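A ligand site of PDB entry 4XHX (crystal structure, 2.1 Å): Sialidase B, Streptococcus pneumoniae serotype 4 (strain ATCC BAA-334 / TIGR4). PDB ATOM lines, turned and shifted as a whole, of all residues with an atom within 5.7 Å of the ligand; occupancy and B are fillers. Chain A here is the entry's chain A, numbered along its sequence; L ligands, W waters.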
ATOM      1  N   ARG A 207      24.588 -24.151  -6.879  1.00  0.00           N
ATOM      2  CA  ARG A 207      23.283 -23.506  -6.924  1.00  0.00           C
ATOM      3  C   ARG A 207      23.483 -21.993  -6.933  1.00  0.00           C
ATOM      4  O   ARG A 207      24.582 -21.509  -6.687  1.00  0.00           O
ATOM      5  CB  ARG A 207      22.438 -23.900  -5.711  1.00  0.00           C
ATOM      6  CG  ARG A 207      21.682 -25.209  -5.864  1.00  0.00           C
ATOM      7  CD  ARG A 207      20.411 -25.193  -4.988  1.00  0.00           C
ATOM      8  NE  ARG A 207      19.485 -24.133  -5.376  1.00  0.00           N
ATOM      9  CZ  ARG A 207      18.377 -23.831  -4.681  1.00  0.00           C
ATOM     10  NH1 ARG A 207      18.089 -24.507  -3.578  1.00  0.00           N
ATOM     11  NH2 ARG A 207      17.567 -22.858  -5.097  1.00  0.00           N
ATOM     12  N   ILE A 208      22.388 -21.272  -7.152  1.00  0.00           N
ATOM     13  CA  ILE A 208      22.372 -19.819  -7.033  1.00  0.00           C
ATOM     14  C   ILE A 208      23.322 -19.104  -8.029  1.00  0.00           C
ATOM     15  O   ILE A 208      24.213 -18.369  -7.620  1.00  0.00           O
ATOM     16  CB  ILE A 208      22.677 -19.374  -5.559  1.00  0.00           C
ATOM     17  CG1 ILE A 208      22.092 -20.349  -4.505  1.00  0.00           C
ATOM     18  CG2 ILE A 208      22.178 -17.980  -5.306  1.00  0.00           C
ATOM     19  CD1 ILE A 208      20.565 -20.553  -4.554  1.00  0.00           C
ATOM     20  N   ASP A 232      20.958 -25.934   1.221  1.00  0.00           N
ATOM     21  CA  ASP A 232      21.259 -24.608   1.810  1.00  0.00           C
ATOM     22  C   ASP A 232      22.060 -24.815   3.100  1.00  0.00           C
ATOM     23  O   ASP A 232      21.961 -25.867   3.726  1.00  0.00           O
ATOM     24  CB  ASP A 232      19.966 -23.875   2.201  1.00  0.00           C
ATOM     25  CG  ASP A 232      19.215 -23.281   1.022  1.00  0.00           C
ATOM     26  OD1 ASP A 232      19.676 -23.388  -0.130  1.00  0.00           O
ATOM     27  OD2 ASP A 232      18.150 -22.689   1.269  1.00  0.00           O
ATOM     28  N   SER A 233      22.822 -23.805   3.526  1.00  0.00           N
ATOM     29  CA  SER A 233      23.436 -23.833   4.861  1.00  0.00           C
ATOM     30  C   SER A 233      22.410 -24.229   5.953  1.00  0.00           C
ATOM     31  O   SER A 233      21.245 -23.898   5.825  1.00  0.00           O
ATOM     32  CB  SER A 233      24.050 -22.464   5.183  1.00  0.00           C
ATOM     33  OG  SER A 233      24.814 -21.995   4.087  1.00  0.00           O
ATOM     34  N   LYS A 234      22.819 -24.925   7.020  1.00  0.00           N
ATOM     35  CA  LYS A 234      24.201 -25.329   7.325  1.00  0.00           C
ATOM     36  C   LYS A 234      24.783 -26.370   6.368  1.00  0.00           C
ATOM     37  O   LYS A 234      24.144 -27.360   6.023  1.00  0.00           O
ATOM     38  CB  LYS A 234      24.281 -25.847   8.773  1.00  0.00           C
ATOM     39  CG  LYS A 234      23.622 -27.213   8.980  1.00  0.00           C
ATOM     40  CD  LYS A 234      23.450 -27.575  10.449  1.00  0.00           C
ATOM     41  CE  LYS A 234      22.624 -28.857  10.584  1.00  0.00           C
ATOM     42  NZ  LYS A 234      22.504 -29.380  11.993  1.00  0.00           N
ATOM     43  N   ILE A 288      26.582 -18.147   1.274  1.00  0.00           N
ATOM     44  CA  ILE A 288      25.412 -18.537   0.502  1.00  0.00           C
ATOM     45  C   ILE A 288      24.773 -17.293  -0.078  1.00  0.00           C
ATOM     46  O   ILE A 288      24.788 -16.240   0.549  1.00  0.00           O
ATOM     47  CB  ILE A 288      24.409 -19.347   1.377  1.00  0.00           C
ATOM     48  CG1 ILE A 288      23.137 -19.713   0.602  1.00  0.00           C
ATOM     49  CG2 ILE A 288      24.069 -18.601   2.654  1.00  0.00           C
ATOM     50  CD1 ILE A 288      22.231 -20.717   1.361  1.00  0.00           C
ATOM     51  N   ASP A 289      24.264 -17.405  -1.305  1.00  0.00           N
ATOM     52  CA  ASP A 289      23.585 -16.311  -1.996  1.00  0.00           C
ATOM     53  C   ASP A 289      24.508 -15.123  -2.276  1.00  0.00           C
ATOM     54  O   ASP A 289      24.696 -14.245  -1.445  1.00  0.00           O
ATOM     55  CB  ASP A 289      22.338 -15.851  -1.246  1.00  0.00           C
ATOM     56  CG  ASP A 289      21.220 -16.892  -1.234  1.00  0.00           C
ATOM     57  OD1 ASP A 289      21.353 -17.947  -1.910  1.00  0.00           O
ATOM     58  OD2 ASP A 289      20.208 -16.662  -0.563  1.00  0.00           O
ATOM     59  N   ASP A 306      25.794 -13.743   1.774  1.00  0.00           N
ATOM     60  CA  ASP A 306      25.516 -14.038   3.181  1.00  0.00           C
ATOM     61  C   ASP A 306      26.659 -14.881   3.773  1.00  0.00           C
ATOM     62  O   ASP A 306      27.267 -15.688   3.079  1.00  0.00           O
ATOM     63  CB  ASP A 306      24.204 -14.824   3.358  1.00  0.00           C
ATOM     64  CG  ASP A 306      22.955 -14.081   2.823  1.00  0.00           C
ATOM     65  OD1 ASP A 306      22.920 -12.833   2.728  1.00  0.00           O
ATOM     66  OD2 ASP A 306      21.988 -14.788   2.482  1.00  0.00           O
ATOM     67  N   MET A 308      27.703 -17.449   7.156  1.00  0.00           N
ATOM     68  CA  MET A 308      27.167 -18.263   8.236  1.00  0.00           C
ATOM     69  C   MET A 308      28.282 -18.893   9.043  1.00  0.00           C
ATOM     70  O   MET A 308      29.139 -19.572   8.491  1.00  0.00           O
ATOM     71  CB  MET A 308      26.303 -19.396   7.662  1.00  0.00           C
ATOM     72  CG  MET A 308      25.250 -18.954   6.664  1.00  0.00           C
ATOM     73  SD  MET A 308      23.773 -18.404   7.515  1.00  0.00           S
ATOM     74  CE  MET A 308      22.958 -17.505   6.208  1.00  0.00           C
ATOM     75  N   ILE A 312      25.490 -23.123  11.129  1.00  0.00           N
ATOM     76  CA  ILE A 312      24.359 -22.190  11.026  1.00  0.00           C
ATOM     77  C   ILE A 312      23.793 -22.000   9.625  1.00  0.00           C
ATOM     78  O   ILE A 312      24.538 -21.826   8.651  1.00  0.00           O
ATOM     79  CB  ILE A 312      24.703 -20.809  11.623  1.00  0.00           C
ATOM     80  CG1 ILE A 312      25.235 -20.962  13.045  1.00  0.00           C
ATOM     81  CG2 ILE A 312      23.488 -19.886  11.567  1.00  0.00           C
ATOM     82  CD1 ILE A 312      24.265 -21.628  13.983  1.00  0.00           C
ATOM     83  N   GLY A 313      22.468 -22.057   9.534  1.00  0.00           N
ATOM     84  CA  GLY A 313      21.735 -21.634   8.351  1.00  0.00           C
ATOM     85  C   GLY A 313      20.633 -20.685   8.808  1.00  0.00           C
ATOM     86  O   GLY A 313      20.526 -20.402  10.001  1.00  0.00           O
ATOM     87  N   ASN A 314      19.824 -20.188   7.870  1.00  0.00           N
ATOM     88  CA  ASN A 314      18.729 -19.272   8.239  1.00  0.00           C
ATOM     89  C   ASN A 314      17.733 -19.916   9.215  1.00  0.00           C
ATOM     90  O   ASN A 314      17.119 -19.235  10.034  1.00  0.00           O
ATOM     91  CB  ASN A 314      18.031 -18.705   6.998  1.00  0.00           C
ATOM     92  CG  ASN A 314      17.175 -19.734   6.267  1.00  0.00           C
ATOM     93  OD1 ASN A 314      17.361 -20.943   6.420  1.00  0.00           O
ATOM     94  ND2 ASN A 314      16.218 -19.256   5.468  1.00  0.00           N
ATOM     95  N   ASN A 315      17.599 -21.236   9.118  1.00  0.00           N
ATOM     96  CA  ASN A 315      16.779 -22.036  10.034  1.00  0.00           C
ATOM     97  C   ASN A 315      17.090 -21.779  11.512  1.00  0.00           C
ATOM     98  O   ASN A 315      16.249 -21.293  12.271  1.00  0.00           O
ATOM     99  CB  ASN A 315      16.957 -23.521   9.719  1.00  0.00           C
ATOM    100  CG  ASN A 315      16.214 -24.417  10.691  1.00  0.00           C
ATOM    101  OD1 ASN A 315      15.023 -24.217  10.959  1.00  0.00           O
ATOM    102  ND2 ASN A 315      16.915 -25.390  11.255  1.00  0.00           N
ATOM    103  N   TYR A 451      18.756 -10.762   4.454  1.00  0.00           N
ATOM    104  CA  TYR A 451      19.226 -11.809   3.567  1.00  0.00           C
ATOM    105  C   TYR A 451      19.483 -11.232   2.190  1.00  0.00           C
ATOM    106  O   TYR A 451      18.595 -10.601   1.611  1.00  0.00           O
ATOM    107  CB  TYR A 451      18.194 -12.946   3.522  1.00  0.00           C
ATOM    108  CG  TYR A 451      18.185 -13.718   4.825  1.00  0.00           C
ATOM    109  CD1 TYR A 451      19.117 -14.717   5.055  1.00  0.00           C
ATOM    110  CD2 TYR A 451      17.283 -13.409   5.833  1.00  0.00           C
ATOM    111  CE1 TYR A 451      19.148 -15.404   6.225  1.00  0.00           C
ATOM    112  CE2 TYR A 451      17.304 -14.097   7.026  1.00  0.00           C
ATOM    113  CZ  TYR A 451      18.236 -15.103   7.215  1.00  0.00           C
ATOM    114  OH  TYR A 451      18.288 -15.820   8.390  1.00  0.00           O
ATOM    115  N   TYR A 471      16.427  -8.854   1.871  1.00  0.00           N
ATOM    116  CA  TYR A 471      15.083  -9.030   2.421  1.00  0.00           C
ATOM    117  C   TYR A 471      15.110  -9.487   3.868  1.00  0.00           C
ATOM    118  O   TYR A 471      16.059 -10.121   4.328  1.00  0.00           O
ATOM    119  CB  TYR A 471      14.233  -9.991   1.572  1.00  0.00           C
ATOM    120  CG  TYR A 471      14.712 -11.439   1.570  1.00  0.00           C
ATOM    121  CD1 TYR A 471      14.272 -12.356   2.530  1.00  0.00           C
ATOM    122  CD2 TYR A 471      15.599 -11.879   0.602  1.00  0.00           C
ATOM    123  CE1 TYR A 471      14.718 -13.676   2.515  1.00  0.00           C
ATOM    124  CE2 TYR A 471      16.046 -13.176   0.588  1.00  0.00           C
ATOM    125  CZ  TYR A 471      15.611 -14.075   1.533  1.00  0.00           C
ATOM    126  OH  TYR A 471      16.086 -15.368   1.468  1.00  0.00           O
ATOM    127  N   THR A 501      10.357 -15.284   1.491  1.00  0.00           N
ATOM    128  CA  THR A 501      11.700 -15.296   0.937  1.00  0.00           C
ATOM    129  C   THR A 501      11.631 -14.345  -0.256  1.00  0.00           C
ATOM    130  O   THR A 501      11.506 -14.774  -1.407  1.00  0.00           O
ATOM    131  CB  THR A 501      12.078 -16.734   0.518  1.00  0.00           C
ATOM    132  OG1 THR A 501      11.916 -17.593   1.654  1.00  0.00           O
ATOM    133  CG2 THR A 501      13.516 -16.813   0.048  1.00  0.00           C
ATOM    134  N   GLU A 503      13.073 -12.643  -2.571  1.00  0.00           N
ATOM    135  CA  GLU A 503      14.234 -12.457  -3.427  1.00  0.00           C
ATOM    136  C   GLU A 503      13.848 -11.479  -4.515  1.00  0.00           C
ATOM    137  O   GLU A 503      12.891 -11.707  -5.272  1.00  0.00           O
ATOM    138  CB  GLU A 503      14.697 -13.804  -3.990  1.00  0.00           C
ATOM    139  CG  GLU A 503      15.303 -14.735  -2.929  1.00  0.00           C
ATOM    140  CD  GLU A 503      15.316 -16.193  -3.338  1.00  0.00           C
ATOM    141  OE1 GLU A 503      16.095 -16.975  -2.744  1.00  0.00           O
ATOM    142  OE2 GLU A 503      14.537 -16.564  -4.248  1.00  0.00           O
ATOM    143  N   ARG A 519       9.999 -12.312  -5.567  1.00  0.00           N
ATOM    144  CA  ARG A 519       9.365 -13.555  -5.131  1.00  0.00           C
ATOM    145  C   ARG A 519       8.445 -13.293  -3.952  1.00  0.00           C
ATOM    146  O   ARG A 519       8.786 -12.520  -3.064  1.00  0.00           O
ATOM    147  CB  ARG A 519      10.462 -14.526  -4.711  1.00  0.00           C
ATOM    148  CG  ARG A 519       9.984 -15.888  -4.208  1.00  0.00           C
ATOM    149  CD  ARG A 519      11.193 -16.729  -3.833  1.00  0.00           C
ATOM    150  NE  ARG A 519      10.844 -17.912  -3.068  1.00  0.00           N
ATOM    151  CZ  ARG A 519      11.709 -18.895  -2.820  1.00  0.00           C
ATOM    152  NH1 ARG A 519      12.955 -18.820  -3.269  1.00  0.00           N
ATOM    153  NH2 ARG A 519      11.322 -19.956  -2.117  1.00  0.00           N
ATOM    154  N   GLY A 552       7.293 -20.120  -4.238  1.00  0.00           N
ATOM    155  CA  GLY A 552       7.928 -19.145  -5.124  1.00  0.00           C
ATOM    156  C   GLY A 552       9.350 -19.500  -5.525  1.00  0.00           C
ATOM    157  O   GLY A 552       9.950 -20.439  -4.990  1.00  0.00           O
ATOM    158  N   ARG A 581       9.047 -26.204  -9.851  1.00  0.00           N
ATOM    159  CA  ARG A 581      10.053 -25.355 -10.499  1.00  0.00           C
ATOM    160  C   ARG A 581      10.375 -25.966 -11.854  1.00  0.00           C
ATOM    161  O   ARG A 581      11.296 -26.782 -12.010  1.00  0.00           O
ATOM    162  CB  ARG A 581      11.285 -25.197  -9.615  1.00  0.00           C
ATOM    163  CG  ARG A 581      10.965 -24.495  -8.293  1.00  0.00           C
ATOM    164  CD  ARG A 581      12.213 -24.132  -7.498  1.00  0.00           C
ATOM    165  NE  ARG A 581      11.912 -23.128  -6.469  1.00  0.00           N
ATOM    166  CZ  ARG A 581      12.678 -22.893  -5.414  1.00  0.00           C
ATOM    167  NH1 ARG A 581      13.798 -23.582  -5.227  1.00  0.00           N
ATOM    168  NH2 ARG A 581      12.321 -21.964  -4.530  1.00  0.00           N
ATOM    169  N   TYR A 615      16.244 -21.345  -9.966  1.00  0.00           N
ATOM    170  CA  TYR A 615      16.940 -20.052  -9.882  1.00  0.00           C
ATOM    171  C   TYR A 615      17.648 -19.790 -11.187  1.00  0.00           C
ATOM    172  O   TYR A 615      18.096 -20.724 -11.858  1.00  0.00           O
ATOM    173  CB  TYR A 615      17.959 -20.054  -8.749  1.00  0.00           C
ATOM    174  CG  TYR A 615      17.383 -19.797  -7.378  1.00  0.00           C
ATOM    175  CD1 TYR A 615      16.232 -20.437  -6.943  1.00  0.00           C
ATOM    176  CD2 TYR A 615      18.027 -18.938  -6.492  1.00  0.00           C
ATOM    177  CE1 TYR A 615      15.712 -20.223  -5.677  1.00  0.00           C
ATOM    178  CE2 TYR A 615      17.517 -18.717  -5.208  1.00  0.00           C
ATOM    179  CZ  TYR A 615      16.359 -19.368  -4.808  1.00  0.00           C
ATOM    180  OH  TYR A 615      15.814 -19.171  -3.549  1.00  0.00           O
ATOM    181  N   SER A 635      14.867 -27.375  -7.929  1.00  0.00           N
ATOM    182  CA  SER A 635      15.693 -27.221  -6.722  1.00  0.00           C
ATOM    183  C   SER A 635      14.859 -27.117  -5.433  1.00  0.00           C
ATOM    184  O   SER A 635      15.395 -26.765  -4.380  1.00  0.00           O
ATOM    185  CB  SER A 635      16.612 -26.007  -6.864  1.00  0.00           C
ATOM    186  OG  SER A 635      15.870 -24.798  -6.893  1.00  0.00           O
ATOM    187  N   TRP A 636      13.566 -27.394  -5.532  1.00  0.00           N
ATOM    188  CA  TRP A 636      12.679 -27.474  -4.360  1.00  0.00           C
ATOM    189  C   TRP A 636      12.343 -28.920  -4.081  1.00  0.00           C
ATOM    190  O   TRP A 636      12.282 -29.341  -2.926  1.00  0.00           O
ATOM    191  CB  TRP A 636      11.378 -26.697  -4.581  1.00  0.00           C
ATOM    192  CG  TRP A 636      10.506 -26.619  -3.342  1.00  0.00           C
ATOM    193  CD1 TRP A 636       9.465 -27.459  -2.994  1.00  0.00           C
ATOM    194  CD2 TRP A 636      10.584 -25.637  -2.286  1.00  0.00           C
ATOM    195  NE1 TRP A 636       8.913 -27.061  -1.804  1.00  0.00           N
ATOM    196  CE2 TRP A 636       9.571 -25.947  -1.357  1.00  0.00           C
ATOM    197  CE3 TRP A 636      11.415 -24.532  -2.056  1.00  0.00           C
ATOM    198  CZ2 TRP A 636       9.361 -25.186  -0.191  1.00  0.00           C
ATOM    199  CZ3 TRP A 636      11.204 -23.772  -0.890  1.00  0.00           C
ATOM    200  CH2 TRP A 636      10.180 -24.111   0.019  1.00  0.00           C
HETATM  201  C1  LIG L   1      20.342 -17.593   3.175  1.00  0.00           C
HETATM  202  C2  LIG L   1      20.679 -18.667   4.058  1.00  0.00           C
HETATM  203  C3  LIG L   1      19.205 -17.719   2.345  1.00  0.00           C
HETATM  204  C4  LIG L   1      18.767 -19.958   3.303  1.00  0.00           C
HETATM  205  C5  LIG L   1      16.257 -20.315  -0.297  1.00  0.00           C
HETATM  206  C6  LIG L   1      16.464 -21.358  -1.366  1.00  0.00           C
HETATM  207  C7  LIG L   1      17.192 -19.041   1.529  1.00  0.00           C
HETATM  208  C8  LIG L   1      19.905 -19.828   4.120  1.00  0.00           C
HETATM  209  C9  LIG L   1      18.413 -18.879   2.421  1.00  0.00           C
HETATM  210  N1  LIG L   1      17.437 -19.983   0.461  1.00  0.00           N
HETATM  211  O1  LIG L   1      13.860 -21.482  -2.173  1.00  0.00           O
HETATM  212  O2  LIG L   1      14.717 -23.246  -0.715  1.00  0.00           O
HETATM  213  O3  LIG L   1      15.378 -23.199  -3.020  1.00  0.00           O
HETATM  214  S1  LIG L   1      15.040 -22.378  -1.858  1.00  0.00           S
HETATM  215 CL1  LIG L   1      20.326 -21.126   5.201  1.00  0.00          CL
HETATM  216  O   HOH W   1      20.035 -14.729   1.050  1.00  0.00           O
HETATM  217  O   HOH W   2      19.419 -19.918  -1.501  1.00  0.00           O
HETATM  218  O   HOH W   3      17.565 -16.309  -0.615  1.00  0.00           O
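The guanidinium group of Arg 581 lies within hydrogen-bond range of the backbone carbonyl oxygen of Gly 552 (2.9 Å).
OH of Tyr 615 sits at hydrogen-bond distance from NH1 of Arg 519, 2.9 Å away.
NH1 of Arg 581 is in hydrogen-bond range of OG of Ser 635.
The backbone NH (N) of Asp 306 sits at hydrogen-bond distance from the backbone carbonyl oxygen (O) of Asp 289 (3.4 Å).
The guanidinium group (NH1) of Arg 207 is in salt-bridge range of the side-chain carboxylate (OD1) of Asp 232, at 3.96 Å.
OE2 of Glu 503 sits at hydrogen-bond distance from OH of Tyr 615 (3.0 Å).
The guanidinium group (NH2) of Arg 519 lies close to the backbone carbonyl oxygen (O) of Gly 552 (3.2 Å).
OG of Ser 635 is in hydrogen-bond range of NH2 of Arg 207, at 3.1 Å.
Water W2 lies within hydrogen-bond range of N1 of the ligand (2.8 Å) and OD1 of Asp 289 (2.8 Å).
Water W1 bridges the side-chain carboxylate of Asp 306 (2.4 Å) and the side-chain carboxylate of Asp 289 (2.5 Å).
Water W3 lies within hydrogen-bond range of the side-chain carboxylate of Asp 289 (2.7 Å), the side-chain carboxylate of Glu 503 (2.7 Å) and the side-chain hydroxyl of Tyr 471 (2.7 Å).
Ser 233 touches the ligand (O to CL1, 3.0 Å).
CG2 of Ile 288 touches C2 of the ligand, at 3.7 Å.
OD2 of Asp 289 touches C3 of the ligand (3.3 Å).
OD2 of Asp 306 touches C1 of the ligand, 3.3 Å away.
Met 308 touches the ligand.
Gly 313 touches the ligand (CA to CL1, 3.5 Å).
Asn 314 touches the ligand (N to CL1, 2.9 Å).
CD1 of Tyr 451 touches C1 of the ligand (3.6 Å).
Tyr 471 touches the ligand (OH to C7, 3.8 Å).
Ser 635 touches the ligand.
CZ3 of Trp 636 touches O2 of the ligand, 3.6 Å away.
Hydrophobic or aromatic side chains within 4 Å of the ligand: Ile 288, Met 308, Tyr 451, Tyr 615 and Trp 636.
16 residues have an atom within 4 Å of the ligand: Arg 207, Asp 232, Ser 233, Ile 288, Asp 289, Asp 306, Met 308, Gly 313, Asn 314, Tyr 451, Tyr 471, Arg 519, Arg 581, Tyr 615, Ser 635 and Trp 636.
The side-chain hydroxyl of Tyr 615 sits close to an oxygen (O1) of the ligand (3.3 Å).
The guanidinium group (NH1) of Arg 581 lies within salt-bridge range of an oxygen (O3) of the ligand (2.7 Å).
O3 of the ligand lies within salt-bridge range of NH2 of Arg 207, at 3.0 Å.
N1 of the ligand lies within salt-bridge range of OD2 of Asp 232 (2.9 Å).
NH2 of Arg 519 is in salt-bridge range of O1 of the ligand, at 3.0 Å.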
